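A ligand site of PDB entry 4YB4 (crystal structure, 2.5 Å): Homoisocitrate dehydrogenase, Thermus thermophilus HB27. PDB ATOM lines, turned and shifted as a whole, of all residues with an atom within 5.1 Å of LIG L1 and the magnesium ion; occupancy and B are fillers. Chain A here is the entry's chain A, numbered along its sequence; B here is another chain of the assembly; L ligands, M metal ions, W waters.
The side-chain amino group of Lys 171 of chain B lies within salt-bridge range of an oxygen (O5) of LIG L1 (2.5 Å). The side-chain hydroxyl (OH) of Tyr 125 is in hydrogen-bond range of an oxygen (O5) of LIG L1 (2.6 Å). The side-chain hydroxyl of Ser 72 sits at hydrogen-bond distance from an oxygen (O6) of LIG L1 (2.7 Å). An oxygen (O4) of LIG L1 is in salt-bridge range of the guanidinium group (NH1) of Arg 88 (2.7 Å). The guanidinium group (NH2) of Arg 98 is in salt-bridge range of an oxygen (O1) of LIG L1 (3.7 Å). NH1 of Arg 118 is in salt-bridge range of O4 of LIG L1, 2.8 Å away. The side-chain amide nitrogen (ND2) of Asn 173 of chain B lies within hydrogen-bond range of an oxygen (O6) of LIG L1 (2.9 Å). O7 of LIG L1 lies within salt-bridge range of NE of Arg 85. The backbone NH (N) of Ser 72 lies within hydrogen-bond range of an oxygen (O12) of LG2 L2 (3.1 Å). O12 of LG2 L2 lies within hydrogen-bond range of O of Ser 72, 3.3 Å away. An oxygen (O13) of LG2 L2 is in hydrogen-bond range of the side-chain hydroxyl of Ser 72. The side-chain amide nitrogen (ND2) of Asn 173 of chain B sits at hydrogen-bond distance from an oxygen (O13) of LG2 L2. OE1 of Glu 257 sits at hydrogen-bond distance from N7 of LG2 L2, 2.7 Å away.
An oxygen (O6) of LIG L1 is in hydrogen-bond range of an oxygen (O13) of LG2 L2.
The side-chain carboxylate (OD2) of Asp 228 is in salt-bridge range of the side-chain amino group (NZ) of Lys 171 of chain B (2.9 Å). OD1 of Asp 228 lies close to NH1 of Arg 98, at 3.96 Å. The side-chain carboxylate (OD1) of Asp 228 lies close to the guanidinium group (NH1) of Arg 118 (3.7 Å). The side-chain amino group (NZ) of Lys 171 of chain B sits close to the side-chain carboxylate (OD2) of Asp 204 of chain B, at 3.9 Å. OH of Tyr 125 sits at hydrogen-bond distance from NZ of Lys 171 of chain B, at 3.5 Å. The guanidinium group (NH2) of Arg 88 is in salt-bridge range of the side-chain carboxylate (OE2) of Glu 257, 2.9 Å away. O of Asn 173 of chain B sits at hydrogen-bond distance from NH1 of Arg 85 (3.4 Å).
Residues that only touch LIG L1: Val 174 of chain B (3.6 Å). 11 residues have an atom within 4 Å of LIG L1: Ser 72, Arg 85, Arg 88, Arg 98, Arg 118, Tyr 125, Asp 228, Lys 171 of chain B, Asn 173 of chain B, Val 174 of chain B and Asp 204 of chain B. Along chain A the residues within 4 Å of LIG L1 span positions 72 to 228.
Merely in contact with the magnesium ion: Arg 98 and Asp 232. Of the 16 residues printed, 4 come within 4 Å of the magnesium ion. Along chain A the residues within 4 Å of the magnesium ion span positions 98 to 232. The nearest printed residue that does not touch the magnesium ion is Lys 171 of chain B (4.3 Å).
The magnesium ion is bound by OD1 of Asp 228 (1.9 Å). OD2 of Asp 204 of chain B is bound to the magnesium ion. The magnesium ion is bound by water W2 (2.1 Å). The magnesium ion is bound by water W1 (2.1 Å). The magnesium ion is bound by an oxygen (O2) of LIG L1, at 2.1 Å. The magnesium ion is bound by O3 of LIG L1 (2.3 Å). The magnesium ion has six donor atoms within binding distance.
Water W2 bridges the backbone carbonyl oxygen of Val 259 and the side-chain carboxylate of Asp 232. Water W1 lies within hydrogen-bond range of the side-chain carboxylate of Asp 232 (2.6 Å), the backbone carbonyl oxygen of Asp 228 (2.6 Å) and the guanidinium group of Arg 98 (2.9 Å). Water W4 lies within hydrogen-bond range of the side-chain amide nitrogen (ND2) of Asn 173 of chain B (3.1 Å) and the side-chain amino group (NZ) of Lys 171 of chain B (3.2 Å). Water W3 lies within hydrogen-bond range of an oxygen (O7) of LIG L1 (2.7 Å), the backbone NH (N) of Arg 85 (3.2 Å) and the backbone NH (N) of Ile 84 (3.4 Å). Water W5 lies within hydrogen-bond range of N7 of LG2 L2, O1 of LIG L1, OE1 of Glu 257 and O of Val 259.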
ATOM      1  N   SER A  72       2.125 -21.499  13.339  1.00  0.00           N
ATOM      2  CA  SER A  72       1.396 -21.209  14.561  1.00  0.00           C
ATOM      3  C   SER A  72       0.681 -19.874  14.416  1.00  0.00           C
ATOM      4  O   SER A  72       1.181 -18.959  13.761  1.00  0.00           O
ATOM      5  CB  SER A  72       2.320 -21.208  15.771  1.00  0.00           C
ATOM      6  OG  SER A  72       3.308 -20.217  15.621  1.00  0.00           O
ATOM      7  N   GLY A  82       2.247 -24.575  20.188  1.00  0.00           N
ATOM      8  CA  GLY A  82       3.275 -24.544  19.162  1.00  0.00           C
ATOM      9  C   GLY A  82       4.058 -25.823  19.220  1.00  0.00           C
ATOM     10  O   GLY A  82       4.498 -26.243  20.304  1.00  0.00           O
ATOM     11  N   ILE A  84       7.063 -27.199  17.780  1.00  0.00           N
ATOM     12  CA  ILE A  84       8.491 -27.317  18.073  1.00  0.00           C
ATOM     13  C   ILE A  84       8.764 -26.883  19.505  1.00  0.00           C
ATOM     14  O   ILE A  84       9.584 -27.468  20.189  1.00  0.00           O
ATOM     15  CB  ILE A  84       9.377 -26.528  17.064  1.00  0.00           C
ATOM     16  CG1 ILE A  84      10.839 -26.948  17.174  1.00  0.00           C
ATOM     17  CG2 ILE A  84       9.285 -25.017  17.289  1.00  0.00           C
ATOM     18  CD1 ILE A  84      11.118 -28.345  16.652  1.00  0.00           C
ATOM     19  N   ARG A  85       8.033 -25.887  19.986  1.00  0.00           N
ATOM     20  CA  ARG A  85       8.216 -25.439  21.346  1.00  0.00           C
ATOM     21  C   ARG A  85       7.782 -26.499  22.343  1.00  0.00           C
ATOM     22  O   ARG A  85       8.428 -26.665  23.378  1.00  0.00           O
ATOM     23  CB  ARG A  85       7.478 -24.112  21.588  1.00  0.00           C
ATOM     24  CG  ARG A  85       8.279 -22.906  21.124  1.00  0.00           C
ATOM     25  CD  ARG A  85       7.650 -21.588  21.560  1.00  0.00           C
ATOM     26  NE  ARG A  85       6.339 -21.410  20.967  1.00  0.00           N
ATOM     27  CZ  ARG A  85       5.190 -21.309  21.637  1.00  0.00           C
ATOM     28  NH1 ARG A  85       4.046 -21.169  20.972  1.00  0.00           N
ATOM     29  NH2 ARG A  85       5.163 -21.342  22.973  1.00  0.00           N
ATOM     30  N   ARG A  88      10.620 -29.073  22.281  1.00  0.00           N
ATOM     31  CA  ARG A  88      11.777 -28.506  22.998  1.00  0.00           C
ATOM     32  C   ARG A  88      11.667 -28.674  24.513  1.00  0.00           C
ATOM     33  O   ARG A  88      12.608 -29.138  25.165  1.00  0.00           O
ATOM     34  CB  ARG A  88      11.946 -27.021  22.657  1.00  0.00           C
ATOM     35  CG  ARG A  88      12.494 -26.745  21.265  1.00  0.00           C
ATOM     36  CD  ARG A  88      12.467 -25.251  20.943  1.00  0.00           C
ATOM     37  NE  ARG A  88      12.860 -25.059  19.555  1.00  0.00           N
ATOM     38  CZ  ARG A  88      12.677 -23.955  18.838  1.00  0.00           C
ATOM     39  NH1 ARG A  88      12.157 -22.862  19.376  1.00  0.00           N
ATOM     40  NH2 ARG A  88      13.032 -23.944  17.561  1.00  0.00           N
ATOM     41  N   ARG A  98      23.096 -22.904  16.610  1.00  0.00           N
ATOM     42  CA  ARG A  98      22.694 -22.173  15.431  1.00  0.00           C
ATOM     43  C   ARG A  98      23.925 -21.489  14.760  1.00  0.00           C
ATOM     44  O   ARG A  98      24.220 -20.330  15.047  1.00  0.00           O
ATOM     45  CB  ARG A  98      21.658 -21.156  15.890  1.00  0.00           C
ATOM     46  CG  ARG A  98      20.316 -21.258  15.224  1.00  0.00           C
ATOM     47  CD  ARG A  98      19.177 -21.643  16.148  1.00  0.00           C
ATOM     48  NE  ARG A  98      18.139 -20.640  16.041  1.00  0.00           N
ATOM     49  CZ  ARG A  98      16.824 -20.827  15.933  1.00  0.00           C
ATOM     50  NH1 ARG A  98      16.066 -19.759  15.849  1.00  0.00           N
ATOM     51  NH2 ARG A  98      16.254 -22.014  15.947  1.00  0.00           N
ATOM     52  N   ARG A 118      21.645 -20.883  21.875  1.00  0.00           N
ATOM     53  CA  ARG A 118      20.552 -20.277  22.600  1.00  0.00           C
ATOM     54  C   ARG A 118      19.880 -21.216  23.582  1.00  0.00           C
ATOM     55  O   ARG A 118      19.568 -22.361  23.254  1.00  0.00           O
ATOM     56  CB  ARG A 118      19.561 -19.551  21.664  1.00  0.00           C
ATOM     57  CG  ARG A 118      18.334 -20.299  21.195  1.00  0.00           C
ATOM     58  CD  ARG A 118      17.064 -19.457  21.154  1.00  0.00           C
ATOM     59  NE  ARG A 118      16.288 -19.828  19.991  1.00  0.00           N
ATOM     60  CZ  ARG A 118      14.971 -19.729  19.840  1.00  0.00           C
ATOM     61  NH1 ARG A 118      14.459 -20.135  18.687  1.00  0.00           N
ATOM     62  NH2 ARG A 118      14.152 -19.265  20.781  1.00  0.00           N
ATOM     63  N   TYR A 125       9.864 -18.148  27.102  1.00  0.00           N
ATOM     64  CA  TYR A 125       9.249 -19.316  26.425  1.00  0.00           C
ATOM     65  C   TYR A 125       8.637 -20.312  27.404  1.00  0.00           C
ATOM     66  O   TYR A 125       8.157 -21.389  27.039  1.00  0.00           O
ATOM     67  CB  TYR A 125      10.270 -20.028  25.526  1.00  0.00           C
ATOM     68  CG  TYR A 125      10.497 -19.313  24.236  1.00  0.00           C
ATOM     69  CD1 TYR A 125      10.956 -17.983  24.222  1.00  0.00           C
ATOM     70  CD2 TYR A 125      10.244 -19.930  23.014  1.00  0.00           C
ATOM     71  CE1 TYR A 125      11.149 -17.305  23.034  1.00  0.00           C
ATOM     72  CE2 TYR A 125      10.445 -19.258  21.823  1.00  0.00           C
ATOM     73  CZ  TYR A 125      10.893 -17.954  21.840  1.00  0.00           C
ATOM     74  OH  TYR A 125      11.092 -17.297  20.675  1.00  0.00           O
ATOM     75  N   ASP A 228      16.677 -16.105  19.601  1.00  0.00           N
ATOM     76  CA  ASP A 228      15.768 -16.169  18.462  1.00  0.00           C
ATOM     77  C   ASP A 228      16.006 -14.997  17.518  1.00  0.00           C
ATOM     78  O   ASP A 228      16.102 -15.160  16.297  1.00  0.00           O
ATOM     79  CB  ASP A 228      14.325 -16.150  18.946  1.00  0.00           C
ATOM     80  CG  ASP A 228      13.335 -16.129  17.800  1.00  0.00           C
ATOM     81  OD1 ASP A 228      13.409 -17.031  16.927  1.00  0.00           O
ATOM     82  OD2 ASP A 228      12.503 -15.180  17.767  1.00  0.00           O
ATOM     83  N   ASP A 232      18.165 -15.081  13.595  1.00  0.00           N
ATOM     84  CA  ASP A 232      17.615 -14.631  12.307  1.00  0.00           C
ATOM     85  C   ASP A 232      18.425 -13.447  11.726  1.00  0.00           C
ATOM     86  O   ASP A 232      18.584 -13.325  10.503  1.00  0.00           O
ATOM     87  CB  ASP A 232      16.128 -14.245  12.395  1.00  0.00           C
ATOM     88  CG  ASP A 232      15.177 -15.411  12.041  1.00  0.00           C
ATOM     89  OD1 ASP A 232      15.489 -16.583  12.396  1.00  0.00           O
ATOM     90  OD2 ASP A 232      14.101 -15.160  11.436  1.00  0.00           O
ATOM     91  N   GLU A 257      16.629 -29.025  12.617  1.00  0.00           N
ATOM     92  CA  GLU A 257      15.645 -28.277  11.845  1.00  0.00           C
ATOM     93  C   GLU A 257      16.261 -26.974  11.347  1.00  0.00           C
ATOM     94  O   GLU A 257      17.142 -26.395  11.991  1.00  0.00           O
ATOM     95  CB  GLU A 257      14.400 -27.940  12.699  1.00  0.00           C
ATOM     96  CG  GLU A 257      14.658 -26.919  13.784  1.00  0.00           C
ATOM     97  CD  GLU A 257      13.416 -26.504  14.544  1.00  0.00           C
ATOM     98  OE1 GLU A 257      12.331 -26.489  13.953  1.00  0.00           O
ATOM     99  OE2 GLU A 257      13.530 -26.164  15.753  1.00  0.00           O
ATOM    100  N   VAL A 259      16.462 -23.023  10.765  1.00  0.00           N
ATOM    101  CA  VAL A 259      16.024 -21.850  11.522  1.00  0.00           C
ATOM    102  C   VAL A 259      14.690 -21.311  11.008  1.00  0.00           C
ATOM    103  O   VAL A 259      13.899 -20.757  11.784  1.00  0.00           O
ATOM    104  CB  VAL A 259      17.116 -20.766  11.473  1.00  0.00           C
ATOM    105  CG1 VAL A 259      16.631 -19.470  12.075  1.00  0.00           C
ATOM    106  CG2 VAL A 259      18.348 -21.258  12.200  1.00  0.00           C
ATOM    107  N   LYS B 171       6.034 -10.825  18.722  1.00  0.00           N
ATOM    108  CA  LYS B 171       6.123 -12.276  18.938  1.00  0.00           C
ATOM    109  C   LYS B 171       4.813 -12.892  19.488  1.00  0.00           C
ATOM    110  O   LYS B 171       4.843 -13.727  20.378  1.00  0.00           O
ATOM    111  CB  LYS B 171       7.295 -12.610  19.865  1.00  0.00           C
ATOM    112  CG  LYS B 171       8.509 -13.100  19.117  1.00  0.00           C
ATOM    113  CD  LYS B 171       8.508 -14.601  18.898  1.00  0.00           C
ATOM    114  CE  LYS B 171       9.246 -14.938  17.615  1.00  0.00           C
ATOM    115  NZ  LYS B 171       9.830 -16.299  17.579  1.00  0.00           N
ATOM    116  N   ASN B 173       2.977 -15.008  18.192  1.00  0.00           N
ATOM    117  CA  ASN B 173       3.061 -16.444  17.963  1.00  0.00           C
ATOM    118  C   ASN B 173       3.521 -17.226  19.200  1.00  0.00           C
ATOM    119  O   ASN B 173       2.941 -18.251  19.516  1.00  0.00           O
ATOM    120  CB  ASN B 173       3.894 -16.786  16.664  1.00  0.00           C
ATOM    121  CG  ASN B 173       5.386 -16.267  16.694  1.00  0.00           C
ATOM    122  OD1 ASN B 173       5.700 -15.198  17.244  1.00  0.00           O
ATOM    123  ND2 ASN B 173       6.283 -17.022  16.035  1.00  0.00           N
ATOM    124  N   VAL B 174       4.497 -16.757  19.955  1.00  0.00           N
ATOM    125  CA  VAL B 174       4.831 -17.503  21.163  1.00  0.00           C
ATOM    126  C   VAL B 174       4.194 -16.911  22.431  1.00  0.00           C
ATOM    127  O   VAL B 174       4.022 -17.643  23.416  1.00  0.00           O
ATOM    128  CB  VAL B 174       6.349 -17.836  21.318  1.00  0.00           C
ATOM    129  CG1 VAL B 174       7.066 -17.772  19.986  1.00  0.00           C
ATOM    130  CG2 VAL B 174       7.044 -16.955  22.314  1.00  0.00           C
ATOM    131  N   ASP B 204      11.786 -11.732  14.757  1.00  0.00           N
ATOM    132  CA  ASP B 204      13.023 -12.366  14.253  1.00  0.00           C
ATOM    133  C   ASP B 204      13.148 -12.209  12.733  1.00  0.00           C
ATOM    134  O   ASP B 204      14.217 -11.843  12.231  1.00  0.00           O
ATOM    135  CB  ASP B 204      13.168 -13.840  14.693  1.00  0.00           C
ATOM    136  CG  ASP B 204      11.959 -14.716  14.338  1.00  0.00           C
ATOM    137  OD1 ASP B 204      10.888 -14.194  13.949  1.00  0.00           O
ATOM    138  OD2 ASP B 204      12.095 -15.954  14.474  1.00  0.00           O
HETATM  139  O1  LIG L   1      12.562 -21.485  16.214  1.00  0.00           O
HETATM  140  C1  LIG L   1      12.417 -20.328  15.845  1.00  0.00           C
HETATM  141  O2  LIG L   1      13.353 -19.552  15.647  1.00  0.00           O
HETATM  142  C2  LIG L   1      10.975 -19.782  15.659  1.00  0.00           C
HETATM  143  O3  LIG L   1      10.994 -18.354  15.548  1.00  0.00           O
HETATM  144  C3  LIG L   1      10.094 -20.222  16.860  1.00  0.00           C
HETATM  145  C4  LIG L   1      10.734 -19.634  18.133  1.00  0.00           C
HETATM  146  O4  LIG L   1      11.690 -20.294  18.615  1.00  0.00           O
HETATM  147  O5  LIG L   1      10.302 -18.541  18.542  1.00  0.00           O
HETATM  148  C5  LIG L   1       8.648 -19.768  16.678  1.00  0.00           C
HETATM  149  C6  LIG L   1       7.807 -20.839  17.414  1.00  0.00           C
HETATM  150  C7  LIG L   1       6.275 -20.642  17.294  1.00  0.00           C
HETATM  151  O6  LIG L   1       5.823 -19.853  16.422  1.00  0.00           O
HETATM  152  O7  LIG L   1       5.583 -21.308  18.095  1.00  0.00           O
HETATM  153  P1  LG2 L   2       9.651 -17.701   7.888  1.00  0.00           P
HETATM  154  O1  LG2 L   2      10.908 -18.238   8.441  1.00  0.00           O
HETATM  155  O2  LG2 L   2       8.743 -18.888   7.434  1.00  0.00           O
HETATM  156  O3  LG2 L   2       9.999 -16.803   6.613  1.00  0.00           O
HETATM  157  C1  LG2 L   2      10.462 -15.471   6.729  1.00  0.00           C
HETATM  158  C2  LG2 L   2      10.854 -15.092   5.298  1.00  0.00           C
HETATM  159  O4  LG2 L   2      11.980 -15.919   4.867  1.00  0.00           O
HETATM  160  C3  LG2 L   2       9.691 -15.381   4.347  1.00  0.00           C
HETATM  161  O5  LG2 L   2       9.498 -14.311   3.446  1.00  0.00           O
HETATM  162  C4  LG2 L   2      10.121 -16.661   3.621  1.00  0.00           C
HETATM  163  O6  LG2 L   2       9.575 -16.693   2.320  1.00  0.00           O
HETATM  164  C5  LG2 L   2      11.639 -16.591   3.626  1.00  0.00           C
HETATM  165  N1  LG2 L   2      12.194 -17.971   3.703  1.00  0.00           N
HETATM  166  C6  LG2 L   2      12.225 -18.748   4.778  1.00  0.00           C
HETATM  167  N2  LG2 L   2      12.728 -19.936   4.450  1.00  0.00           N
HETATM  168  C7  LG2 L   2      13.021 -19.894   3.149  1.00  0.00           C
HETATM  169  C8  LG2 L   2      13.570 -20.801   2.304  1.00  0.00           C
HETATM  170  N3  LG2 L   2      13.915 -21.984   2.785  1.00  0.00           N
HETATM  171  N4  LG2 L   2      13.767 -20.516   1.017  1.00  0.00           N
HETATM  172  C9  LG2 L   2      13.396 -19.257   0.554  1.00  0.00           C
HETATM  173  N5  LG2 L   2      12.851 -18.342   1.428  1.00  0.00           N
HETATM  174  C10 LG2 L   2      12.678 -18.674   2.702  1.00  0.00           C
HETATM  175  O7  LG2 L   2       9.060 -16.884   9.129  1.00  0.00           O
HETATM  176  P2  LG2 L   2       7.691 -16.189   9.328  1.00  0.00           P
HETATM  177  O8  LG2 L   2       7.196 -15.762   7.905  1.00  0.00           O
HETATM  178  O9  LG2 L   2       7.783 -15.061  10.294  1.00  0.00           O
HETATM  179  O10 LG2 L   2       6.618 -17.248   9.928  1.00  0.00           O
HETATM  180  C11 LG2 L   2       6.108 -18.361   9.202  1.00  0.00           C
HETATM  181  C12 LG2 L   2       5.490 -19.341  10.166  1.00  0.00           C
HETATM  182  O11 LG2 L   2       6.484 -20.268  10.637  1.00  0.00           O
HETATM  183  C13 LG2 L   2       4.903 -18.708  11.417  1.00  0.00           C
HETATM  184  O12 LG2 L   2       3.681 -19.394  11.647  1.00  0.00           O
HETATM  185  C14 LG2 L   2       5.892 -19.005  12.532  1.00  0.00           C
HETATM  186  O13 LG2 L   2       5.185 -19.076  13.791  1.00  0.00           O
HETATM  187  C15 LG2 L   2       6.395 -20.362  12.082  1.00  0.00           C
HETATM  188  N6  LG2 L   2       7.769 -20.773  12.420  1.00  0.00           N
HETATM  189  C16 LG2 L   2       7.993 -22.092  12.774  1.00  0.00           C
HETATM  190  C17 LG2 L   2       9.251 -22.609  13.047  1.00  0.00           C
HETATM  191  C18 LG2 L   2       9.384 -23.961  13.441  1.00  0.00           C
HETATM  192  O14 LG2 L   2       8.425 -24.713  13.593  1.00  0.00           O
HETATM  193  N7  LG2 L   2      10.613 -24.411  13.705  1.00  0.00           N
HETATM  194  C19 LG2 L   2      10.388 -21.774  12.883  1.00  0.00           C
HETATM  195  C20 LG2 L   2      10.134 -20.442  12.487  1.00  0.00           C
HETATM  196  C21 LG2 L   2       8.864 -19.938  12.250  1.00  0.00           C
HETATM  197 MG    MG M   1      13.113 -17.539  15.089  1.00  0.00          MG
HETATM  198  O   HOH W   1      15.163 -17.161  14.881  1.00  0.00           O
HETATM  199  O   HOH W   2      13.085 -18.238  13.161  1.00  0.00           O
HETATM  200  O   HOH W   3       6.240 -23.911  18.289  1.00  0.00           O
HETATM  201  O   HOH W   4       9.033 -17.120  14.598  1.00  0.00           O
HETATM  202  O   HOH W   5      13.201 -23.318  14.053  1.00  0.00           O
